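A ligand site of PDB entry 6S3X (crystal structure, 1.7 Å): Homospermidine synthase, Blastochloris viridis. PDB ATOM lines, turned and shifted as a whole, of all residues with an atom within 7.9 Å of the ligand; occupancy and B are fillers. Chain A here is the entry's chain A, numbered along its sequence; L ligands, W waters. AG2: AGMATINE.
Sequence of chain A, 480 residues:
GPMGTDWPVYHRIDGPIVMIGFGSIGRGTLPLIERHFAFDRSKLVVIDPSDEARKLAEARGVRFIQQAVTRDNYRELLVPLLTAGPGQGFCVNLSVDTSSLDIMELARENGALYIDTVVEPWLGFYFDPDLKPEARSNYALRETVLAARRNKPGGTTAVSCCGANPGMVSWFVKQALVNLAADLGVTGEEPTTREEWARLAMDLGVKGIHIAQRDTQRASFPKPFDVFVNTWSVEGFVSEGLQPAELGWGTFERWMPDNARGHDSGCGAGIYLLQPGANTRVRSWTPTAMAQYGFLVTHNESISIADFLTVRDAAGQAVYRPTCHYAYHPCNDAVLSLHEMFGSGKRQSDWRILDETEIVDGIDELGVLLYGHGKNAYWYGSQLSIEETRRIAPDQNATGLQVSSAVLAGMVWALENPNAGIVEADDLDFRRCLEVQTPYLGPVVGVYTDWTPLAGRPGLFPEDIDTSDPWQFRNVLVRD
NH1 of Arg 149 touches CA of the ligand (3.5 Å).
Arg 194 touches the ligand.
Phe 308 touches the ligand (CD1 to NH2, 3.5 Å).
The nearest printed residue that does not touch the ligand is Arg 142 (4.04 Å).
The side-chain carboxylate (OD1) of Asp 427 is in salt-bridge range of a nitrogen (NH2) of the ligand (3.0 Å).
The side-chain carboxylate of Asp 307 is in salt-bridge range of a nitrogen (NH1) of the ligand.
Water W2 lies within hydrogen-bond range of NH2 of the ligand (2.7 Å), O of Ser 304 (2.9 Å), OE1 of Glu 424 (3.0 Å) and NH2 of Arg 142 (3.4 Å).
Water W3 lies within hydrogen-bond range of O of Ile 422, O of Ala 420 and N of the ligand.
Water W1 lies within hydrogen-bond range of OD2 of Asp 427 (2.8 Å), OE1 of Glu 424 (2.8 Å), NH2 of Arg 149 (2.8 Å) and NH2 of the ligand (3.0 Å).
NH1 of Arg 149 is in salt-bridge range of OD2 of Asp 427 (3.6 Å).
The backbone NH (N) of Glu 424 is in hydrogen-bond range of the side-chain carboxylate (OD2) of Asp 427.
The guanidinium group (NH2) of Arg 142 is in salt-bridge range of the side-chain carboxylate (OD2) of Asp 307 (2.8 Å).
O of Asp 307 lies within hydrogen-bond range of OG1 of Thr 310.
NH2 of Arg 194 is in salt-bridge range of OE2 of Glu 195 (2.5 Å).
The backbone carbonyl oxygen of Ile 422 lies within hydrogen-bond range of the guanidinium group of Arg 149 (3.0 Å).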
ATOM      1  N   ARG A 142      19.006  -2.842  25.072  1.00  0.00           N
ATOM      2  CA  ARG A 142      18.253  -3.936  24.494  1.00  0.00           C
ATOM      3  C   ARG A 142      18.749  -4.278  23.100  1.00  0.00           C
ATOM      4  O   ARG A 142      18.786  -5.465  22.714  1.00  0.00           O
ATOM      5  CB  ARG A 142      16.766  -3.586  24.482  1.00  0.00           C
ATOM      6  CG  ARG A 142      15.911  -4.535  23.690  1.00  0.00           C
ATOM      7  CD  ARG A 142      14.451  -4.177  23.831  1.00  0.00           C
ATOM      8  NE  ARG A 142      13.600  -5.176  23.190  1.00  0.00           N
ATOM      9  CZ  ARG A 142      13.122  -5.075  21.953  1.00  0.00           C
ATOM     10  NH1 ARG A 142      13.397  -4.011  21.207  1.00  0.00           N
ATOM     11  NH2 ARG A 142      12.356  -6.043  21.457  1.00  0.00           N
ATOM     12  N   LEU A 146      19.466  -7.770  21.134  1.00  0.00           N
ATOM     13  CA  LEU A 146      18.953  -8.128  19.819  1.00  0.00           C
ATOM     14  C   LEU A 146      20.078  -8.424  18.840  1.00  0.00           C
ATOM     15  O   LEU A 146      19.968  -9.338  18.015  1.00  0.00           O
ATOM     16  CB  LEU A 146      18.053  -7.012  19.267  1.00  0.00           C
ATOM     17  CG  LEU A 146      16.888  -6.537  20.154  1.00  0.00           C
ATOM     18  CD1 LEU A 146      15.897  -5.646  19.374  1.00  0.00           C
ATOM     19  CD2 LEU A 146      16.159  -7.726  20.789  1.00  0.00           C
ATOM     20  N   ARG A 149      21.382 -11.957  19.457  1.00  0.00           N
ATOM     21  CA  ARG A 149      20.489 -12.962  18.891  1.00  0.00           C
ATOM     22  C   ARG A 149      20.677 -13.081  17.381  1.00  0.00           C
ATOM     23  O   ARG A 149      20.635 -14.195  16.839  1.00  0.00           O
ATOM     24  CB  ARG A 149      19.037 -12.621  19.208  1.00  0.00           C
ATOM     25  CG  ARG A 149      18.055 -13.534  18.498  1.00  0.00           C
ATOM     26  CD  ARG A 149      16.722 -13.490  19.183  1.00  0.00           C
ATOM     27  NE  ARG A 149      16.036 -12.221  18.985  1.00  0.00           N
ATOM     28  CZ  ARG A 149      15.087 -11.747  19.800  1.00  0.00           C
ATOM     29  NH1 ARG A 149      14.724 -12.438  20.870  1.00  0.00           N
ATOM     30  NH2 ARG A 149      14.510 -10.588  19.542  1.00  0.00           N
ATOM     31  N   GLY A 154      19.123 -19.168  17.632  1.00  0.00           N
ATOM     32  CA  GLY A 154      18.880 -20.449  18.271  1.00  0.00           C
ATOM     33  C   GLY A 154      19.920 -20.705  19.357  1.00  0.00           C
ATOM     34  O   GLY A 154      20.544 -19.782  19.890  1.00  0.00           O
ATOM     35  N   LYS A 174      -0.960  -9.889  26.592  1.00  0.00           N
ATOM     36  CA  LYS A 174      -1.611 -10.872  25.739  1.00  0.00           C
ATOM     37  C   LYS A 174      -2.985 -11.262  26.277  1.00  0.00           C
ATOM     38  O   LYS A 174      -3.951 -11.357  25.511  1.00  0.00           O
ATOM     39  CB  LYS A 174      -0.727 -12.103  25.588  1.00  0.00           C
ATOM     40  CG  LYS A 174       0.482 -11.875  24.676  1.00  0.00           C
ATOM     41  CD  LYS A 174       1.219 -13.173  24.425  1.00  0.00           C
ATOM     42  CE  LYS A 174       2.290 -13.001  23.361  1.00  0.00           C
ATOM     43  NZ  LYS A 174       3.554 -12.429  23.911  1.00  0.00           N
ATOM     44  N   ARG A 194       3.964 -13.755  16.594  1.00  0.00           N
ATOM     45  CA  ARG A 194       4.132 -12.328  16.836  1.00  0.00           C
ATOM     46  C   ARG A 194       3.275 -11.476  15.893  1.00  0.00           C
ATOM     47  O   ARG A 194       2.645 -10.502  16.311  1.00  0.00           O
ATOM     48  CB  ARG A 194       5.608 -11.946  16.697  1.00  0.00           C
ATOM     49  CG  ARG A 194       5.871 -10.482  16.824  1.00  0.00           C
ATOM     50  CD  ARG A 194       7.356 -10.222  16.692  1.00  0.00           C
ATOM     51  NE  ARG A 194       7.954 -10.893  15.546  1.00  0.00           N
ATOM     52  CZ  ARG A 194       7.955 -10.410  14.307  1.00  0.00           C
ATOM     53  NH1 ARG A 194       7.380  -9.240  14.057  1.00  0.00           N
ATOM     54  NH2 ARG A 194       8.531 -11.085  13.327  1.00  0.00           N
ATOM     55  N   GLU A 195       3.252 -11.841  14.609  1.00  0.00           N
ATOM     56  CA  GLU A 195       2.524 -11.052  13.621  1.00  0.00           C
ATOM     57  C   GLU A 195       1.015 -11.052  13.871  1.00  0.00           C
ATOM     58  O   GLU A 195       0.329 -10.058  13.591  1.00  0.00           O
ATOM     59  CB  GLU A 195       2.838 -11.596  12.223  1.00  0.00           C
ATOM     60  CG  GLU A 195       4.311 -11.402  11.776  1.00  0.00           C
ATOM     61  CD  GLU A 195       5.324 -12.392  12.388  1.00  0.00           C
ATOM     62  OE1 GLU A 195       4.955 -13.373  13.049  1.00  0.00           O
ATOM     63  OE2 GLU A 195       6.535 -12.157  12.170  1.00  0.00           O
ATOM     64  N   CYS A 267      15.350  -1.388  16.258  1.00  0.00           N
ATOM     65  CA  CYS A 267      14.031  -1.876  15.916  1.00  0.00           C
ATOM     66  C   CYS A 267      13.052  -0.744  15.584  1.00  0.00           C
ATOM     67  O   CYS A 267      12.002  -1.016  14.986  1.00  0.00           O
ATOM     68  CB  CYS A 267      13.491  -2.712  17.068  1.00  0.00           C
ATOM     69  SG  CYS A 267      12.977  -1.779  18.538  1.00  0.00           S
ATOM     70  N   ILE A 303       9.893  -0.627  25.406  1.00  0.00           N
ATOM     71  CA  ILE A 303      10.343  -0.885  24.051  1.00  0.00           C
ATOM     72  C   ILE A 303       9.857  -2.255  23.572  1.00  0.00           C
ATOM     73  O   ILE A 303       9.375  -2.396  22.448  1.00  0.00           O
ATOM     74  CB  ILE A 303      11.880  -0.794  23.972  1.00  0.00           C
ATOM     75  CG1 ILE A 303      12.366   0.504  24.607  1.00  0.00           C
ATOM     76  CG2 ILE A 303      12.332  -0.943  22.529  1.00  0.00           C
ATOM     77  CD1 ILE A 303      11.738   1.752  24.045  1.00  0.00           C
ATOM     78  N   SER A 304      10.042  -3.299  24.390  1.00  0.00           N
ATOM     79  CA  SER A 304       9.876  -4.651  23.880  1.00  0.00           C
ATOM     80  C   SER A 304       8.432  -4.926  23.498  1.00  0.00           C
ATOM     81  O   SER A 304       8.162  -5.593  22.499  1.00  0.00           O
ATOM     82  CB  SER A 304      10.389  -5.680  24.894  1.00  0.00           C
ATOM     83  OG  SER A 304       9.440  -6.031  25.893  1.00  0.00           O
ATOM     84  N   ILE A 305       7.482  -4.373  24.255  1.00  0.00           N
ATOM     85  CA  ILE A 305       6.077  -4.591  23.957  1.00  0.00           C
ATOM     86  C   ILE A 305       5.666  -3.822  22.702  1.00  0.00           C
ATOM     87  O   ILE A 305       4.991  -4.369  21.813  1.00  0.00           O
ATOM     88  CB  ILE A 305       5.206  -4.214  25.176  1.00  0.00           C
ATOM     89  CG1 ILE A 305       5.434  -5.225  26.312  1.00  0.00           C
ATOM     90  CG2 ILE A 305       3.751  -4.140  24.791  1.00  0.00           C
ATOM     91  CD1 ILE A 305       4.830  -4.821  27.652  1.00  0.00           C
ATOM     92  N   ALA A 306       6.075  -2.555  22.591  1.00  0.00           N
ATOM     93  CA  ALA A 306       5.789  -1.791  21.381  1.00  0.00           C
ATOM     94  C   ALA A 306       6.370  -2.473  20.146  1.00  0.00           C
ATOM     95  O   ALA A 306       5.703  -2.572  19.105  1.00  0.00           O
ATOM     96  CB  ALA A 306       6.360  -0.373  21.493  1.00  0.00           C
ATOM     97  N   ASP A 307       7.610  -2.953  20.245  1.00  0.00           N
ATOM     98  CA  ASP A 307       8.272  -3.676  19.158  1.00  0.00           C
ATOM     99  C   ASP A 307       7.478  -4.921  18.781  1.00  0.00           C
ATOM    100  O   ASP A 307       7.159  -5.137  17.609  1.00  0.00           O
ATOM    101  CB  ASP A 307       9.685  -4.055  19.617  1.00  0.00           C
ATOM    102  CG  ASP A 307      10.537  -4.677  18.529  1.00  0.00           C
ATOM    103  OD1 ASP A 307      10.254  -4.461  17.329  1.00  0.00           O
ATOM    104  OD2 ASP A 307      11.500  -5.397  18.881  1.00  0.00           O
ATOM    105  N   PHE A 308       7.147  -5.744  19.783  1.00  0.00           N
ATOM    106  CA  PHE A 308       6.413  -6.985  19.556  1.00  0.00           C
ATOM    107  C   PHE A 308       5.083  -6.724  18.861  1.00  0.00           C
ATOM    108  O   PHE A 308       4.660  -7.534  18.021  1.00  0.00           O
ATOM    109  CB  PHE A 308       6.205  -7.680  20.902  1.00  0.00           C
ATOM    110  CG  PHE A 308       5.535  -9.019  20.808  1.00  0.00           C
ATOM    111  CD1 PHE A 308       6.244 -10.145  20.438  1.00  0.00           C
ATOM    112  CD2 PHE A 308       4.188  -9.149  21.100  1.00  0.00           C
ATOM    113  CE1 PHE A 308       5.638 -11.374  20.341  1.00  0.00           C
ATOM    114  CE2 PHE A 308       3.570 -10.391  21.021  1.00  0.00           C
ATOM    115  CZ  PHE A 308       4.291 -11.505  20.632  1.00  0.00           C
ATOM    116  N   LEU A 309       4.398  -5.636  19.194  1.00  0.00           N
ATOM    117  CA  LEU A 309       3.080  -5.375  18.616  1.00  0.00           C
ATOM    118  C   LEU A 309       3.153  -4.446  17.408  1.00  0.00           C
ATOM    119  O   LEU A 309       2.159  -3.773  17.088  1.00  0.00           O
ATOM    120  CB  LEU A 309       2.122  -4.824  19.664  1.00  0.00           C
ATOM    121  CG  LEU A 309       1.772  -5.786  20.822  1.00  0.00           C
ATOM    122  CD1 LEU A 309       0.935  -5.060  21.874  1.00  0.00           C
ATOM    123  CD2 LEU A 309       1.053  -7.041  20.336  1.00  0.00           C
ATOM    124  N   THR A 310       4.291  -4.396  16.736  1.00  0.00           N
ATOM    125  CA  THR A 310       4.438  -3.593  15.529  1.00  0.00           C
ATOM    126  C   THR A 310       3.962  -4.390  14.323  1.00  0.00           C
ATOM    127  O   THR A 310       4.315  -5.553  14.159  1.00  0.00           O
ATOM    128  CB  THR A 310       5.901  -3.156  15.341  1.00  0.00           C
ATOM    129  OG1 THR A 310       6.298  -2.325  16.444  1.00  0.00           O
ATOM    130  CG2 THR A 310       6.078  -2.383  14.039  1.00  0.00           C
ATOM    131  N   TRP A 413       9.570 -22.468  31.965  1.00  0.00           N
ATOM    132  CA  TRP A 413       9.494 -22.381  30.522  1.00  0.00           C
ATOM    133  C   TRP A 413      10.825 -22.756  29.865  1.00  0.00           C
ATOM    134  O   TRP A 413      10.849 -23.471  28.868  1.00  0.00           O
ATOM    135  CB  TRP A 413       9.067 -20.978  30.099  1.00  0.00           C
ATOM    136  CG  TRP A 413       8.748 -20.954  28.663  1.00  0.00           C
ATOM    137  CD1 TRP A 413       7.551 -21.231  28.085  1.00  0.00           C
ATOM    138  CD2 TRP A 413       9.652 -20.671  27.586  1.00  0.00           C
ATOM    139  NE1 TRP A 413       7.643 -21.137  26.712  1.00  0.00           N
ATOM    140  CE2 TRP A 413       8.923 -20.799  26.379  1.00  0.00           C
ATOM    141  CE3 TRP A 413      11.011 -20.325  27.516  1.00  0.00           C
ATOM    142  CZ2 TRP A 413       9.501 -20.581  25.135  1.00  0.00           C
ATOM    143  CZ3 TRP A 413      11.578 -20.121  26.268  1.00  0.00           C
ATOM    144  CH2 TRP A 413      10.832 -20.239  25.100  1.00  0.00           C
ATOM    145  N   ALA A 420      15.735 -22.584  22.612  1.00  0.00           N
ATOM    146  CA  ALA A 420      14.988 -21.529  21.949  1.00  0.00           C
ATOM    147  C   ALA A 420      15.796 -20.259  21.729  1.00  0.00           C
ATOM    148  O   ALA A 420      15.250 -19.264  21.244  1.00  0.00           O
ATOM    149  CB  ALA A 420      13.729 -21.197  22.759  1.00  0.00           C
ATOM    150  N   GLY A 421      17.089 -20.253  22.071  1.00  0.00           N
ATOM    151  CA  GLY A 421      17.896 -19.054  21.887  1.00  0.00           C
ATOM    152  C   GLY A 421      17.549 -17.947  22.865  1.00  0.00           C
ATOM    153  O   GLY A 421      16.856 -18.139  23.856  1.00  0.00           O
ATOM    154  N   ILE A 422      18.065 -16.769  22.558  1.00  0.00           N
ATOM    155  CA  ILE A 422      17.786 -15.564  23.345  1.00  0.00           C
ATOM    156  C   ILE A 422      16.332 -15.158  23.120  1.00  0.00           C
ATOM    157  O   ILE A 422      15.915 -14.910  21.985  1.00  0.00           O
ATOM    158  CB  ILE A 422      18.746 -14.433  22.952  1.00  0.00           C
ATOM    159  CG1 ILE A 422      20.187 -14.856  23.284  1.00  0.00           C
ATOM    160  CG2 ILE A 422      18.400 -13.139  23.641  1.00  0.00           C
ATOM    161  CD1 ILE A 422      21.249 -13.938  22.720  1.00  0.00           C
ATOM    162  N   VAL A 423      15.568 -15.073  24.213  1.00  0.00           N
ATOM    163  CA  VAL A 423      14.158 -14.695  24.162  1.00  0.00           C
ATOM    164  C   VAL A 423      13.852 -13.664  25.237  1.00  0.00           C
ATOM    165  O   VAL A 423      14.492 -13.622  26.288  1.00  0.00           O
ATOM    166  CB  VAL A 423      13.251 -15.932  24.331  1.00  0.00           C
ATOM    167  CG1 VAL A 423      13.405 -16.845  23.135  1.00  0.00           C
ATOM    168  CG2 VAL A 423      13.588 -16.720  25.589  1.00  0.00           C
ATOM    169  N   GLU A 424      12.866 -12.810  24.947  1.00  0.00           N
ATOM    170  CA  GLU A 424      12.257 -11.925  25.937  1.00  0.00           C
ATOM    171  C   GLU A 424      10.930 -12.504  26.412  1.00  0.00           C
ATOM    172  O   GLU A 424      10.429 -13.489  25.870  1.00  0.00           O
ATOM    173  CB  GLU A 424      12.055 -10.518  25.348  1.00  0.00           C
ATOM    174  CG  GLU A 424      13.321  -9.796  24.929  1.00  0.00           C
ATOM    175  CD  GLU A 424      13.068  -8.436  24.282  1.00  0.00           C
ATOM    176  OE1 GLU A 424      12.339  -8.353  23.269  1.00  0.00           O
ATOM    177  OE2 GLU A 424      13.607  -7.433  24.793  1.00  0.00           O
ATOM    178  N   ALA A 425      10.351 -11.859  27.421  1.00  0.00           N
ATOM    179  CA  ALA A 425       9.087 -12.354  27.975  1.00  0.00           C
ATOM    180  C   ALA A 425       7.983 -12.391  26.926  1.00  0.00           C
ATOM    181  O   ALA A 425       7.095 -13.247  26.983  1.00  0.00           O
ATOM    182  CB  ALA A 425       8.659 -11.491  29.166  1.00  0.00           C
ATOM    183  N   ASP A 426       8.011 -11.456  25.980  1.00  0.00           N
ATOM    184  CA  ASP A 426       7.045 -11.450  24.885  1.00  0.00           C
ATOM    185  C   ASP A 426       7.121 -12.701  24.029  1.00  0.00           C
ATOM    186  O   ASP A 426       6.133 -13.044  23.361  1.00  0.00           O
ATOM    187  CB  ASP A 426       7.290 -10.205  24.019  1.00  0.00           C
ATOM    188  CG  ASP A 426       7.266  -8.953  24.842  1.00  0.00           C
ATOM    189  OD1 ASP A 426       6.167  -8.536  25.246  1.00  0.00           O
ATOM    190  OD2 ASP A 426       8.356  -8.392  25.138  1.00  0.00           O
ATOM    191  N   ASP A 427       8.250 -13.402  24.051  1.00  0.00           N
ATOM    192  CA  ASP A 427       8.434 -14.572  23.221  1.00  0.00           C
ATOM    193  C   ASP A 427       8.056 -15.874  23.901  1.00  0.00           C
ATOM    194  O   ASP A 427       8.041 -16.918  23.235  1.00  0.00           O
ATOM    195  CB  ASP A 427       9.892 -14.693  22.761  1.00  0.00           C
ATOM    196  CG  ASP A 427      10.351 -13.498  22.011  1.00  0.00           C
ATOM    197  OD1 ASP A 427       9.584 -13.086  21.120  1.00  0.00           O
ATOM    198  OD2 ASP A 427      11.437 -12.959  22.313  1.00  0.00           O
ATOM    199  N   LEU A 428       7.786 -15.863  25.211  1.00  0.00           N
ATOM    200  CA  LEU A 428       7.419 -17.100  25.896  1.00  0.00           C
ATOM    201  C   LEU A 428       5.944 -17.413  25.690  1.00  0.00           C
ATOM    202  O   LEU A 428       5.159 -16.557  25.279  1.00  0.00           O
ATOM    203  CB  LEU A 428       7.698 -16.996  27.404  1.00  0.00           C
ATOM    204  CG  LEU A 428       9.002 -16.311  27.804  1.00  0.00           C
ATOM    205  CD1 LEU A 428       9.349 -16.534  29.254  1.00  0.00           C
ATOM    206  CD2 LEU A 428      10.118 -16.830  26.914  1.00  0.00           C
HETATM  207  N   AG2 L   1      12.918 -16.009  18.958  1.00  0.00           N
HETATM  208  CA  AG2 L   1      12.742 -14.585  18.953  1.00  0.00           C
HETATM  209  CB  AG2 L   1      11.572 -14.054  18.127  1.00  0.00           C
HETATM  210  CG  AG2 L   1      11.664 -12.555  17.913  1.00  0.00           C
HETATM  211  CD  AG2 L   1      10.334 -11.851  18.089  1.00  0.00           C
HETATM  212  NE  AG2 L   1      10.453 -10.423  18.087  1.00  0.00           N
HETATM  213  CZ  AG2 L   1      10.138  -9.676  19.128  1.00  0.00           C
HETATM  214  NH1 AG2 L   1      10.177  -8.450  19.053  1.00  0.00           N
HETATM  215  NH2 AG2 L   1       9.768 -10.221  20.252  1.00  0.00           N
HETATM  216  O   HOH W   1      12.523 -10.529  21.517  1.00  0.00           O
HETATM  217  O   HOH W   2       9.650  -8.017  21.870  1.00  0.00           O
HETATM  218  O   HOH W   3      15.494 -16.814  20.138  1.00  0.00           O
HETATM  219  O   HOH W   4      10.716  -8.050  15.802  1.00  0.00           O
